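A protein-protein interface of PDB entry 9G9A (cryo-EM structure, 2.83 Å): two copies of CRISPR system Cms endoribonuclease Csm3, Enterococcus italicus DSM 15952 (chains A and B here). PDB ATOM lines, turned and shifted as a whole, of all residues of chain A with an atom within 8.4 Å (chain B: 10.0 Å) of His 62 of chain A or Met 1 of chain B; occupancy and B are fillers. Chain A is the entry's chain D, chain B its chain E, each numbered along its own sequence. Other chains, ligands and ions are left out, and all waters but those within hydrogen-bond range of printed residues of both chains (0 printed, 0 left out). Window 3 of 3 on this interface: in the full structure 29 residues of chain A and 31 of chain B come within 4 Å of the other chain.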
ATOM      1  N   MET A  55      21.149  14.785  16.867  1.00  0.00           N
ATOM      2  CA  MET A  55      21.977  14.195  17.914  1.00  0.00           C
ATOM      3  C   MET A  55      21.118  13.633  19.039  1.00  0.00           C
ATOM      4  O   MET A  55      21.390  12.544  19.556  1.00  0.00           O
ATOM      5  CB  MET A  55      22.963  15.234  18.450  1.00  0.00           C
ATOM      6  CG  MET A  55      24.075  15.590  17.479  1.00  0.00           C
ATOM      7  SD  MET A  55      25.205  16.824  18.146  1.00  0.00           S
ATOM      8  CE  MET A  55      25.781  15.989  19.619  1.00  0.00           C
ATOM      9  N   ARG A  56      20.073  14.366  19.436  1.00  0.00           N
ATOM     10  CA  ARG A  56      19.183  13.887  20.485  1.00  0.00           C
ATOM     11  C   ARG A  56      18.467  12.613  20.062  1.00  0.00           C
ATOM     12  O   ARG A  56      18.333  11.676  20.856  1.00  0.00           O
ATOM     13  CB  ARG A  56      18.172  14.975  20.847  1.00  0.00           C
ATOM     14  CG  ARG A  56      17.192  14.577  21.936  1.00  0.00           C
ATOM     15  CD  ARG A  56      16.011  15.534  21.985  1.00  0.00           C
ATOM     16  NE  ARG A  56      15.102  15.224  23.081  1.00  0.00           N
ATOM     17  CZ  ARG A  56      15.042  15.901  24.218  1.00  0.00           C
ATOM     18  NH1 ARG A  56      15.820  16.945  24.443  1.00  0.00           N
ATOM     19  NH2 ARG A  56      14.176  15.525  25.153  1.00  0.00           N
ATOM     20  N   SER A  57      18.003  12.558  18.811  1.00  0.00           N
ATOM     21  CA  SER A  57      17.326  11.365  18.314  1.00  0.00           C
ATOM     22  C   SER A  57      18.261  10.163  18.308  1.00  0.00           C
ATOM     23  O   SER A  57      17.883   9.061  18.731  1.00  0.00           O
ATOM     24  CB  SER A  57      16.779  11.627  16.911  1.00  0.00           C
ATOM     25  OG  SER A  57      16.422  10.417  16.268  1.00  0.00           O
ATOM     26  N   LEU A  58      19.493  10.355  17.832  1.00  0.00           N
ATOM     27  CA  LEU A  58      20.438   9.246  17.783  1.00  0.00           C
ATOM     28  C   LEU A  58      20.826   8.781  19.181  1.00  0.00           C
ATOM     29  O   LEU A  58      20.929   7.575  19.434  1.00  0.00           O
ATOM     30  CB  LEU A  58      21.672   9.647  16.978  1.00  0.00           C
ATOM     31  CG  LEU A  58      21.379   9.914  15.501  1.00  0.00           C
ATOM     32  CD1 LEU A  58      22.581  10.512  14.806  1.00  0.00           C
ATOM     33  CD2 LEU A  58      20.938   8.637  14.814  1.00  0.00           C
ATOM     34  N   LEU A  59      21.038   9.719  20.109  1.00  0.00           N
ATOM     35  CA  LEU A  59      21.351   9.339  21.482  1.00  0.00           C
ATOM     36  C   LEU A  59      20.183   8.613  22.138  1.00  0.00           C
ATOM     37  O   LEU A  59      20.387   7.671  22.912  1.00  0.00           O
ATOM     38  CB  LEU A  59      21.742  10.571  22.294  1.00  0.00           C
ATOM     39  CG  LEU A  59      23.228  10.691  22.626  1.00  0.00           C
ATOM     40  CD1 LEU A  59      23.479  11.906  23.496  1.00  0.00           C
ATOM     41  CD2 LEU A  59      23.722   9.430  23.311  1.00  0.00           C
ATOM     42  N   ALA A  60      18.952   9.048  21.861  1.00  0.00           N
ATOM     43  CA  ALA A  60      17.789   8.374  22.424  1.00  0.00           C
ATOM     44  C   ALA A  60      17.646   6.963  21.869  1.00  0.00           C
ATOM     45  O   ALA A  60      17.286   6.037  22.604  1.00  0.00           O
ATOM     46  CB  ALA A  60      16.528   9.194  22.155  1.00  0.00           C
ATOM     47  N   LYS A  61      17.908   6.782  20.572  1.00  0.00           N
ATOM     48  CA  LYS A  61      17.894   5.439  20.002  1.00  0.00           C
ATOM     49  C   LYS A  61      18.984   4.566  20.612  1.00  0.00           C
ATOM     50  O   LYS A  61      18.758   3.384  20.896  1.00  0.00           O
ATOM     51  CB  LYS A  61      18.052   5.501  18.483  1.00  0.00           C
ATOM     52  CG  LYS A  61      16.766   5.782  17.732  1.00  0.00           C
ATOM     53  CD  LYS A  61      16.991   5.712  16.232  1.00  0.00           C
ATOM     54  CE  LYS A  61      15.687   5.847  15.468  1.00  0.00           C
ATOM     55  NZ  LYS A  61      15.899   5.738  13.999  1.00  0.00           N
ATOM     56  N   HIS A  62      20.180   5.126  20.808  1.00  0.00           N
ATOM     57  CA  HIS A  62      21.283   4.347  21.360  1.00  0.00           C
ATOM     58  C   HIS A  62      21.011   3.935  22.801  1.00  0.00           C
ATOM     59  O   HIS A  62      21.134   2.757  23.154  1.00  0.00           O
ATOM     60  CB  HIS A  62      22.583   5.146  21.267  1.00  0.00           C
ATOM     61  CG  HIS A  62      23.713   4.560  22.055  1.00  0.00           C
ATOM     62  ND1 HIS A  62      24.226   5.163  23.183  1.00  0.00           N
ATOM     63  CD2 HIS A  62      24.428   3.423  21.880  1.00  0.00           C
ATOM     64  CE1 HIS A  62      25.207   4.425  23.668  1.00  0.00           C
ATOM     65  NE2 HIS A  62      25.351   3.363  22.895  1.00  0.00           N
ATOM     66  N   ILE A  63      20.638   4.893  23.650  1.00  0.00           N
ATOM     67  CA  ILE A  63      20.401   4.585  25.057  1.00  0.00           C
ATOM     68  C   ILE A  63      19.129   3.763  25.221  1.00  0.00           C
ATOM     69  O   ILE A  63      19.107   2.768  25.953  1.00  0.00           O
ATOM     70  CB  ILE A  63      20.356   5.881  25.884  1.00  0.00           C
ATOM     71  CG1 ILE A  63      21.726   6.563  25.869  1.00  0.00           C
ATOM     72  CG2 ILE A  63      19.907   5.594  27.307  1.00  0.00           C
ATOM     73  CD1 ILE A  63      21.826   7.772  26.769  1.00  0.00           C
ATOM     74  N   GLY A  64      18.059   4.156  24.540  1.00  0.00           N
ATOM     75  CA  GLY A  64      16.799   3.445  24.626  1.00  0.00           C
ATOM     76  C   GLY A  64      16.661   2.364  23.575  1.00  0.00           C
ATOM     77  O   GLY A  64      16.170   2.618  22.475  1.00  0.00           O
ATOM     78  N   ALA A  76      15.399   9.336  28.660  1.00  0.00           N
ATOM     79  CA  ALA A  76      16.404   8.931  29.626  1.00  0.00           C
ATOM     80  C   ALA A  76      17.005  10.154  30.318  1.00  0.00           C
ATOM     81  O   ALA A  76      17.007  11.255  29.761  1.00  0.00           O
ATOM     82  CB  ALA A  76      17.506   8.127  28.940  1.00  0.00           C
ATOM     83  N   ILE A  79      19.623  12.096  28.152  1.00  0.00           N
ATOM     84  CA  ILE A  79      19.122  12.922  27.056  1.00  0.00           C
ATOM     85  C   ILE A  79      18.594  14.249  27.589  1.00  0.00           C
ATOM     86  O   ILE A  79      18.897  15.321  27.053  1.00  0.00           O
ATOM     87  CB  ILE A  79      18.044  12.168  26.257  1.00  0.00           C
ATOM     88  CG1 ILE A  79      18.678  11.127  25.332  1.00  0.00           C
ATOM     89  CG2 ILE A  79      17.187  13.140  25.462  1.00  0.00           C
ATOM     90  CD1 ILE A  79      18.957   9.796  25.991  1.00  0.00           C
ATOM     91  N   GLU A 167      31.239  11.199  26.452  1.00  0.00           N
ATOM     92  CA  GLU A 167      31.117   9.887  25.831  1.00  0.00           C
ATOM     93  C   GLU A 167      29.824   9.805  25.035  1.00  0.00           C
ATOM     94  O   GLU A 167      29.839   9.514  23.831  1.00  0.00           O
ATOM     95  CB  GLU A 167      31.176   8.790  26.895  1.00  0.00           C
ATOM     96  CG  GLU A 167      30.903   7.389  26.366  1.00  0.00           C
ATOM     97  CD  GLU A 167      31.862   6.976  25.266  1.00  0.00           C
ATOM     98  OE1 GLU A 167      31.587   7.277  24.084  1.00  0.00           O
ATOM     99  OE2 GLU A 167      32.895   6.350  25.583  1.00  0.00           O
ATOM    100  N   ASN A 168      28.702  10.142  25.677  1.00  0.00           N
ATOM    101  CA  ASN A 168      27.432  10.191  24.965  1.00  0.00           C
ATOM    102  C   ASN A 168      27.542  11.101  23.752  1.00  0.00           C
ATOM    103  O   ASN A 168      27.191  10.709  22.632  1.00  0.00           O
ATOM    104  CB  ASN A 168      26.318  10.663  25.899  1.00  0.00           C
ATOM    105  CG  ASN A 168      25.950   9.624  26.935  1.00  0.00           C
ATOM    106  OD1 ASN A 168      26.700   8.679  27.173  1.00  0.00           O
ATOM    107  ND2 ASN A 168      24.792   9.793  27.558  1.00  0.00           N
ATOM    108  N   ILE A 169      28.105  12.298  23.949  1.00  0.00           N
ATOM    109  CA  ILE A 169      28.298  13.213  22.830  1.00  0.00           C
ATOM    110  C   ILE A 169      29.101  12.525  21.739  1.00  0.00           C
ATOM    111  O   ILE A 169      28.678  12.465  20.577  1.00  0.00           O
ATOM    112  CB  ILE A 169      28.985  14.507  23.302  1.00  0.00           C
ATOM    113  CG1 ILE A 169      28.091  15.269  24.279  1.00  0.00           C
ATOM    114  CG2 ILE A 169      29.344  15.381  22.113  1.00  0.00           C
ATOM    115  CD1 ILE A 169      28.727  16.526  24.827  1.00  0.00           C
ATOM    116  N   LYS A 170      30.232  11.922  22.121  1.00  0.00           N
ATOM    117  CA  LYS A 170      31.032  11.179  21.158  1.00  0.00           C
ATOM    118  C   LYS A 170      30.169  10.158  20.438  1.00  0.00           C
ATOM    119  O   LYS A 170      30.096  10.147  19.202  1.00  0.00           O
ATOM    120  CB  LYS A 170      32.204  10.495  21.865  1.00  0.00           C
ATOM    121  CG  LYS A 170      32.926   9.467  21.012  1.00  0.00           C
ATOM    122  CD  LYS A 170      33.789   8.545  21.862  1.00  0.00           C
ATOM    123  CE  LYS A 170      34.921   9.301  22.533  1.00  0.00           C
ATOM    124  NZ  LYS A 170      35.866   9.880  21.541  1.00  0.00           N
ATOM    125  N   THR A 171      29.431   9.355  21.210  1.00  0.00           N
ATOM    126  CA  THR A 171      28.552   8.358  20.615  1.00  0.00           C
ATOM    127  C   THR A 171      27.628   9.010  19.600  1.00  0.00           C
ATOM    128  O   THR A 171      27.585   8.605  18.432  1.00  0.00           O
ATOM    129  CB  THR A 171      27.747   7.651  21.706  1.00  0.00           C
ATOM    130  OG1 THR A 171      28.636   7.166  22.719  1.00  0.00           O
ATOM    131  CG2 THR A 171      26.972   6.482  21.124  1.00  0.00           C
ATOM    132  N   ALA A 172      26.953  10.086  20.013  1.00  0.00           N
ATOM    133  CA  ALA A 172      26.030  10.762  19.111  1.00  0.00           C
ATOM    134  C   ALA A 172      26.741  11.171  17.832  1.00  0.00           C
ATOM    135  O   ALA A 172      26.281  10.858  16.726  1.00  0.00           O
ATOM    136  CB  ALA A 172      25.412  11.975  19.805  1.00  0.00           C
ATOM    137  N   LEU A 175      27.302   8.270  15.643  1.00  0.00           N
ATOM    138  CA  LEU A 175      26.053   7.940  14.972  1.00  0.00           C
ATOM    139  C   LEU A 175      25.748   8.955  13.883  1.00  0.00           C
ATOM    140  O   LEU A 175      25.331   8.587  12.778  1.00  0.00           O
ATOM    141  CB  LEU A 175      24.915   7.878  15.990  1.00  0.00           C
ATOM    142  CG  LEU A 175      24.952   6.722  16.991  1.00  0.00           C
ATOM    143  CD1 LEU A 175      24.377   7.149  18.324  1.00  0.00           C
ATOM    144  CD2 LEU A 175      24.184   5.538  16.447  1.00  0.00           C
ATOM    145  N   MET B   1      20.625  -0.161  22.644  1.00  0.00           N
ATOM    146  CA  MET B   1      21.818  -0.275  21.814  1.00  0.00           C
ATOM    147  C   MET B   1      21.478  -0.124  20.336  1.00  0.00           C
ATOM    148  O   MET B   1      20.837  -0.993  19.744  1.00  0.00           O
ATOM    149  CB  MET B   1      22.518  -1.613  22.056  1.00  0.00           C
ATOM    150  CG  MET B   1      23.728  -1.853  21.168  1.00  0.00           C
ATOM    151  SD  MET B   1      25.057  -0.667  21.447  1.00  0.00           S
ATOM    152  CE  MET B   1      25.476  -1.019  23.152  1.00  0.00           C
ATOM    153  N   TYR B   2      21.912   0.984  19.742  1.00  0.00           N
ATOM    154  CA  TYR B   2      21.694   1.248  18.322  1.00  0.00           C
ATOM    155  C   TYR B   2      22.900   0.714  17.561  1.00  0.00           C
ATOM    156  O   TYR B   2      24.030   1.160  17.771  1.00  0.00           O
ATOM    157  CB  TYR B   2      21.489   2.739  18.074  1.00  0.00           C
ATOM    158  CG  TYR B   2      20.905   3.079  16.718  1.00  0.00           C
ATOM    159  CD1 TYR B   2      20.473   2.084  15.851  1.00  0.00           C
ATOM    160  CD2 TYR B   2      20.790   4.399  16.307  1.00  0.00           C
ATOM    161  CE1 TYR B   2      19.943   2.396  14.615  1.00  0.00           C
ATOM    162  CE2 TYR B   2      20.261   4.719  15.073  1.00  0.00           C
ATOM    163  CZ  TYR B   2      19.838   3.714  14.232  1.00  0.00           C
ATOM    164  OH  TYR B   2      19.309   4.029  13.002  1.00  0.00           O
ATOM    165  N   SER B   3      22.661  -0.246  16.674  1.00  0.00           N
ATOM    166  CA  SER B   3      23.714  -0.844  15.866  1.00  0.00           C
ATOM    167  C   SER B   3      23.552  -0.424  14.411  1.00  0.00           C
ATOM    168  O   SER B   3      22.495  -0.641  13.810  1.00  0.00           O
ATOM    169  CB  SER B   3      23.688  -2.367  15.977  1.00  0.00           C
ATOM    170  OG  SER B   3      24.637  -2.942  15.100  1.00  0.00           O
ATOM    171  N   LYS B   4      24.600   0.176  13.854  1.00  0.00           N
ATOM    172  CA  LYS B   4      24.629   0.585  12.457  1.00  0.00           C
ATOM    173  C   LYS B   4      25.693  -0.222  11.730  1.00  0.00           C
ATOM    174  O   LYS B   4      26.866  -0.214  12.130  1.00  0.00           O
ATOM    175  CB  LYS B   4      24.909   2.083  12.327  1.00  0.00           C
ATOM    176  CG  LYS B   4      24.149   2.934  13.327  1.00  0.00           C
ATOM    177  CD  LYS B   4      24.149   4.392  12.929  1.00  0.00           C
ATOM    178  CE  LYS B   4      23.321   4.606  11.681  1.00  0.00           C
ATOM    179  NZ  LYS B   4      23.141   6.048  11.394  1.00  0.00           N
ATOM    180  N   ASN B 155      20.322  -0.092   9.512  1.00  0.00           N
ATOM    181  CA  ASN B 155      20.042   0.251  10.898  1.00  0.00           C
ATOM    182  C   ASN B 155      19.395  -0.947  11.579  1.00  0.00           C
ATOM    183  O   ASN B 155      18.378  -1.463  11.103  1.00  0.00           O
ATOM    184  CB  ASN B 155      19.133   1.475  10.983  1.00  0.00           C
ATOM    185  CG  ASN B 155      19.666   2.649  10.188  1.00  0.00           C
ATOM    186  OD1 ASN B 155      20.477   3.430  10.683  1.00  0.00           O
ATOM    187  ND2 ASN B 155      19.211   2.779   8.947  1.00  0.00           N
ATOM    188  N   VAL B 156      19.983  -1.387  12.690  1.00  0.00           N
ATOM    189  CA  VAL B 156      19.472  -2.537  13.429  1.00  0.00           C
ATOM    190  C   VAL B 156      18.432  -2.018  14.418  1.00  0.00           C
ATOM    191  O   VAL B 156      18.753  -1.670  15.555  1.00  0.00           O
ATOM    192  CB  VAL B 156      20.591  -3.307  14.133  1.00  0.00           C
ATOM    193  CG1 VAL B 156      20.023  -4.484  14.895  1.00  0.00           C
ATOM    194  CG2 VAL B 156      21.618  -3.781  13.118  1.00  0.00           C
ATOM    195  N   GLU B 157      17.176  -1.951  13.978  1.00  0.00           N
ATOM    196  CA  GLU B 157      16.078  -1.589  14.862  1.00  0.00           C
ATOM    197  C   GLU B 157      15.457  -2.800  15.540  1.00  0.00           C
ATOM    198  O   GLU B 157      14.688  -2.636  16.494  1.00  0.00           O
ATOM    199  CB  GLU B 157      14.997  -0.831  14.083  1.00  0.00           C
ATOM    200  CG  GLU B 157      15.524   0.296  13.203  1.00  0.00           C
ATOM    201  CD  GLU B 157      16.046   1.481  13.997  1.00  0.00           C
ATOM    202  OE1 GLU B 157      15.776   1.558  15.213  1.00  0.00           O
ATOM    203  OE2 GLU B 157      16.730   2.340  13.401  1.00  0.00           O
ATOM    204  N   ASN B 158      15.771  -4.003  15.066  1.00  0.00           N
ATOM    205  CA  ASN B 158      15.252  -5.237  15.644  1.00  0.00           C
ATOM    206  C   ASN B 158      16.245  -6.344  15.332  1.00  0.00           C
ATOM    207  O   ASN B 158      16.483  -6.644  14.159  1.00  0.00           O
ATOM    208  CB  ASN B 158      13.869  -5.572  15.085  1.00  0.00           C
ATOM    209  CG  ASN B 158      13.139  -6.605  15.917  1.00  0.00           C
ATOM    210  OD1 ASN B 158      13.380  -7.805  15.789  1.00  0.00           O
ATOM    211  ND2 ASN B 158      12.239  -6.143  16.775  1.00  0.00           N
ATOM    212  N   ILE B 159      16.821  -6.941  16.379  1.00  0.00           N
ATOM    213  CA  ILE B 159      17.879  -7.933  16.193  1.00  0.00           C
ATOM    214  C   ILE B 159      17.367  -9.129  15.400  1.00  0.00           C
ATOM    215  O   ILE B 159      18.072  -9.668  14.538  1.00  0.00           O
ATOM    216  CB  ILE B 159      18.445  -8.366  17.559  1.00  0.00           C
ATOM    217  CG1 ILE B 159      18.981  -7.158  18.329  1.00  0.00           C
ATOM    218  CG2 ILE B 159      19.537  -9.411  17.380  1.00  0.00           C
ATOM    219  CD1 ILE B 159      20.274  -6.605  17.780  1.00  0.00           C
ATOM    220  N   VAL B 162      17.185  -8.911  11.369  1.00  0.00           N
ATOM    221  CA  VAL B 162      18.353  -8.461  10.615  1.00  0.00           C
ATOM    222  C   VAL B 162      18.713  -9.454   9.516  1.00  0.00           C
ATOM    223  O   VAL B 162      19.007  -9.062   8.381  1.00  0.00           O
ATOM    224  CB  VAL B 162      19.541  -8.221  11.563  1.00  0.00           C
ATOM    225  CG1 VAL B 162      20.777  -7.834  10.773  1.00  0.00           C
ATOM    226  CG2 VAL B 162      19.200  -7.141  12.565  1.00  0.00           C
ATOM    227  N   THR B 201      30.040  -3.903  11.261  1.00  0.00           N
ATOM    228  CA  THR B 201      29.186  -3.213  12.225  1.00  0.00           C
ATOM    229  C   THR B 201      29.966  -2.028  12.779  1.00  0.00           C
ATOM    230  O   THR B 201      30.729  -2.165  13.738  1.00  0.00           O
ATOM    231  CB  THR B 201      28.751  -4.159  13.338  1.00  0.00           C
ATOM    232  OG1 THR B 201      28.073  -5.285  12.769  1.00  0.00           O
ATOM    233  CG2 THR B 201      27.821  -3.450  14.304  1.00  0.00           C
ATOM    234  N   VAL B 202      29.777  -0.858  12.170  1.00  0.00           N
ATOM    235  CA  VAL B 202      30.525   0.321  12.594  1.00  0.00           C
ATOM    236  C   VAL B 202      30.050   0.801  13.960  1.00  0.00           C
ATOM    237  O   VAL B 202      30.859   1.217  14.798  1.00  0.00           O
ATOM    238  CB  VAL B 202      30.428   1.431  11.534  1.00  0.00           C
ATOM    239  CG1 VAL B 202      31.275   2.623  11.941  1.00  0.00           C
ATOM    240  CG2 VAL B 202      30.882   0.904  10.194  1.00  0.00           C
ATOM    241  N   VAL B 203      28.743   0.752  14.216  1.00  0.00           N
ATOM    242  CA  VAL B 203      28.191   1.236  15.475  1.00  0.00           C
ATOM    243  C   VAL B 203      27.502   0.084  16.191  1.00  0.00           C
ATOM    244  O   VAL B 203      26.749  -0.680  15.579  1.00  0.00           O
ATOM    245  CB  VAL B 203      27.215   2.410  15.256  1.00  0.00           C
ATOM    246  CG1 VAL B 203      26.625   2.860  16.578  1.00  0.00           C
ATOM    247  CG2 VAL B 203      27.923   3.566  14.574  1.00  0.00           C
ATOM    248  N   GLY B 204      27.770  -0.043  17.483  1.00  0.00           N
ATOM    249  CA  GLY B 204      27.118  -1.036  18.307  1.00  0.00           C
ATOM    250  C   GLY B 204      27.990  -2.241  18.593  1.00  0.00           C
ATOM    251  O   GLY B 204      29.221  -2.199  18.534  1.00  0.00           O
ATOM    252  N   ASP B 205      27.316  -3.345  18.917  1.00  0.00           N
ATOM    253  CA  ASP B 205      27.984  -4.603  19.220  1.00  0.00           C
ATOM    254  C   ASP B 205      27.416  -5.769  18.421  1.00  0.00           C
ATOM    255  O   ASP B 205      27.698  -6.927  18.753  1.00  0.00           O
ATOM    256  CB  ASP B 205      27.898  -4.909  20.720  1.00  0.00           C
ATOM    257  CG  ASP B 205      26.467  -5.040  21.206  1.00  0.00           C
ATOM    258  OD1 ASP B 205      25.563  -4.474  20.559  1.00  0.00           O
ATOM    259  OD2 ASP B 205      26.247  -5.708  22.238  1.00  0.00           O
ATOM    260  N   PHE B 206      26.624  -5.499  17.388  1.00  0.00           N
ATOM    261  CA  PHE B 206      26.060  -6.567  16.574  1.00  0.00           C
ATOM    262  C   PHE B 206      27.161  -7.273  15.794  1.00  0.00           C
ATOM    263  O   PHE B 206      28.127  -6.650  15.347  1.00  0.00           O
ATOM    264  CB  PHE B 206      25.009  -6.003  15.619  1.00  0.00           C
ATOM    265  CG  PHE B 206      24.240  -7.052  14.871  1.00  0.00           C
ATOM    266  CD1 PHE B 206      23.115  -7.632  15.429  1.00  0.00           C
ATOM    267  CD2 PHE B 206      24.637  -7.454  13.608  1.00  0.00           C
ATOM    268  CE1 PHE B 206      22.403  -8.597  14.744  1.00  0.00           C
ATOM    269  CE2 PHE B 206      23.930  -8.417  12.919  1.00  0.00           C
ATOM    270  CZ  PHE B 206      22.813  -8.989  13.487  1.00  0.00           C
ATOM    271  N   ASP B 207      27.014  -8.587  15.639  1.00  0.00           N
ATOM    272  CA  ASP B 207      27.980  -9.407  14.917  1.00  0.00           C
ATOM    273  C   ASP B 207      27.450  -9.652  13.509  1.00  0.00           C
ATOM    274  O   ASP B 207      26.535 -10.458  13.312  1.00  0.00           O
ATOM    275  CB  ASP B 207      28.232 -10.724  15.649  1.00  0.00           C
ATOM    276  CG  ASP B 207      29.460 -11.450  15.135  1.00  0.00           C
ATOM    277  OD1 ASP B 207      30.583 -10.961  15.377  1.00  0.00           O
ATOM    278  OD2 ASP B 207      29.304 -12.508  14.490  1.00  0.00           O
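OH of Tyr 2 of chain B is in hydrogen-bond range of OD1 of Asn 155 of chain B (2.7 Å). OH of Tyr 2 of chain B is in hydrogen-bond range of OE2 of Glu 157 of chain B (3.1 Å). The side-chain hydroxyl (OG) of Ser 3 of chain B lies close to the backbone carbonyl oxygen (O) of Val 203 of chain B (3.1 Å). The backbone NH (N) of Val 202 of chain B lies within hydrogen-bond range of the backbone carbonyl oxygen (O) of Lys 4 of chain B (3.0 Å). The backbone carbonyl oxygen (O) of Val 203 of chain B is in hydrogen-bond range of the backbone NH (N) of Lys 4 of chain B (2.9 Å).
Tyr 2 of chain B touches Leu 58 of chain A. CD of Lys 61 of chain A touches CE2 of Tyr 2 of chain B, 3.6 Å away. His 62 of chain A touches Tyr 2 of chain B (CA to CB, 3.7 Å). CD2 of Leu 175 of chain A touches CD2 of Tyr 2 of chain B, at 3.6 Å. O of Leu 175 of chain A touches NZ of Lys 4 of chain B, 3.6 Å away. Leu 175 of chain A touches Val 203 of chain B (CD2 to CG1, 3.6 Å).
Printed residues of chain B that touch a printed residue of chain A: Met 1, Tyr 2, Lys 4, Glu 157 and Val 203. Hydrophobic or aromatic side chains of chain B that line the printed part of chain A: Tyr 2 and Val 203. Of the 19 printed residues of chain A, 4 touch a printed residue of chain B. Printed residues of chain A that touch a printed residue of chain B: Leu 58, Lys 61, His 62 and Leu 175. Among the printed residues, Asp or Glu carboxylates within 4 Å of a Lys or Arg side-chain nitrogen of the other chain: Lys 61 of chain A with Glu 157 of chain B (3.5 Å).
No position is printed for both chains.
His 62 of chain A touches just these residues of chain B: Met 1 (3.0 Å) and Tyr 2 (3.7 Å). Of chain A, only His 62 (3.0 Å) comes within 4 Å of Met 1 of chain B. No residue of chain B comes within 4 Å of Gly 64 of chain A. Printed residues of chain A within 4 Å of Lys 4 of chain B: Leu 175. Of the printed residues of chain A, Val 203 of chain B touches Leu 175. Printed residues of chain B within 4 Å of Leu 175 of chain A: Tyr 2 (3.6 Å), Lys 4 (3.6 Å) and Val 203 (3.6 Å). Printed residues of chain B within 4 Å of Leu 58 of chain A: Tyr 2. Asp 207 of chain B touches none of the printed residues of chain A. Val 162 of chain B touches none of the printed residues of chain A. The nearest residue of chain B that does not touch His 62 of chain A is Val 203 of chain B (5.8 Å). The nearest residue of chain A that does not touch Met 1 of chain B is Lys 61 of chain A (4.4 Å).
NZ of Lys 61 of chain A lies within salt-bridge range of OE2 of Glu 157 of chain B, at 3.5 Å. The backbone NH (N) of Met 1 of chain B sits at hydrogen-bond distance from the backbone carbonyl oxygen (O) of His 62 of chain A (3.0 Å).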
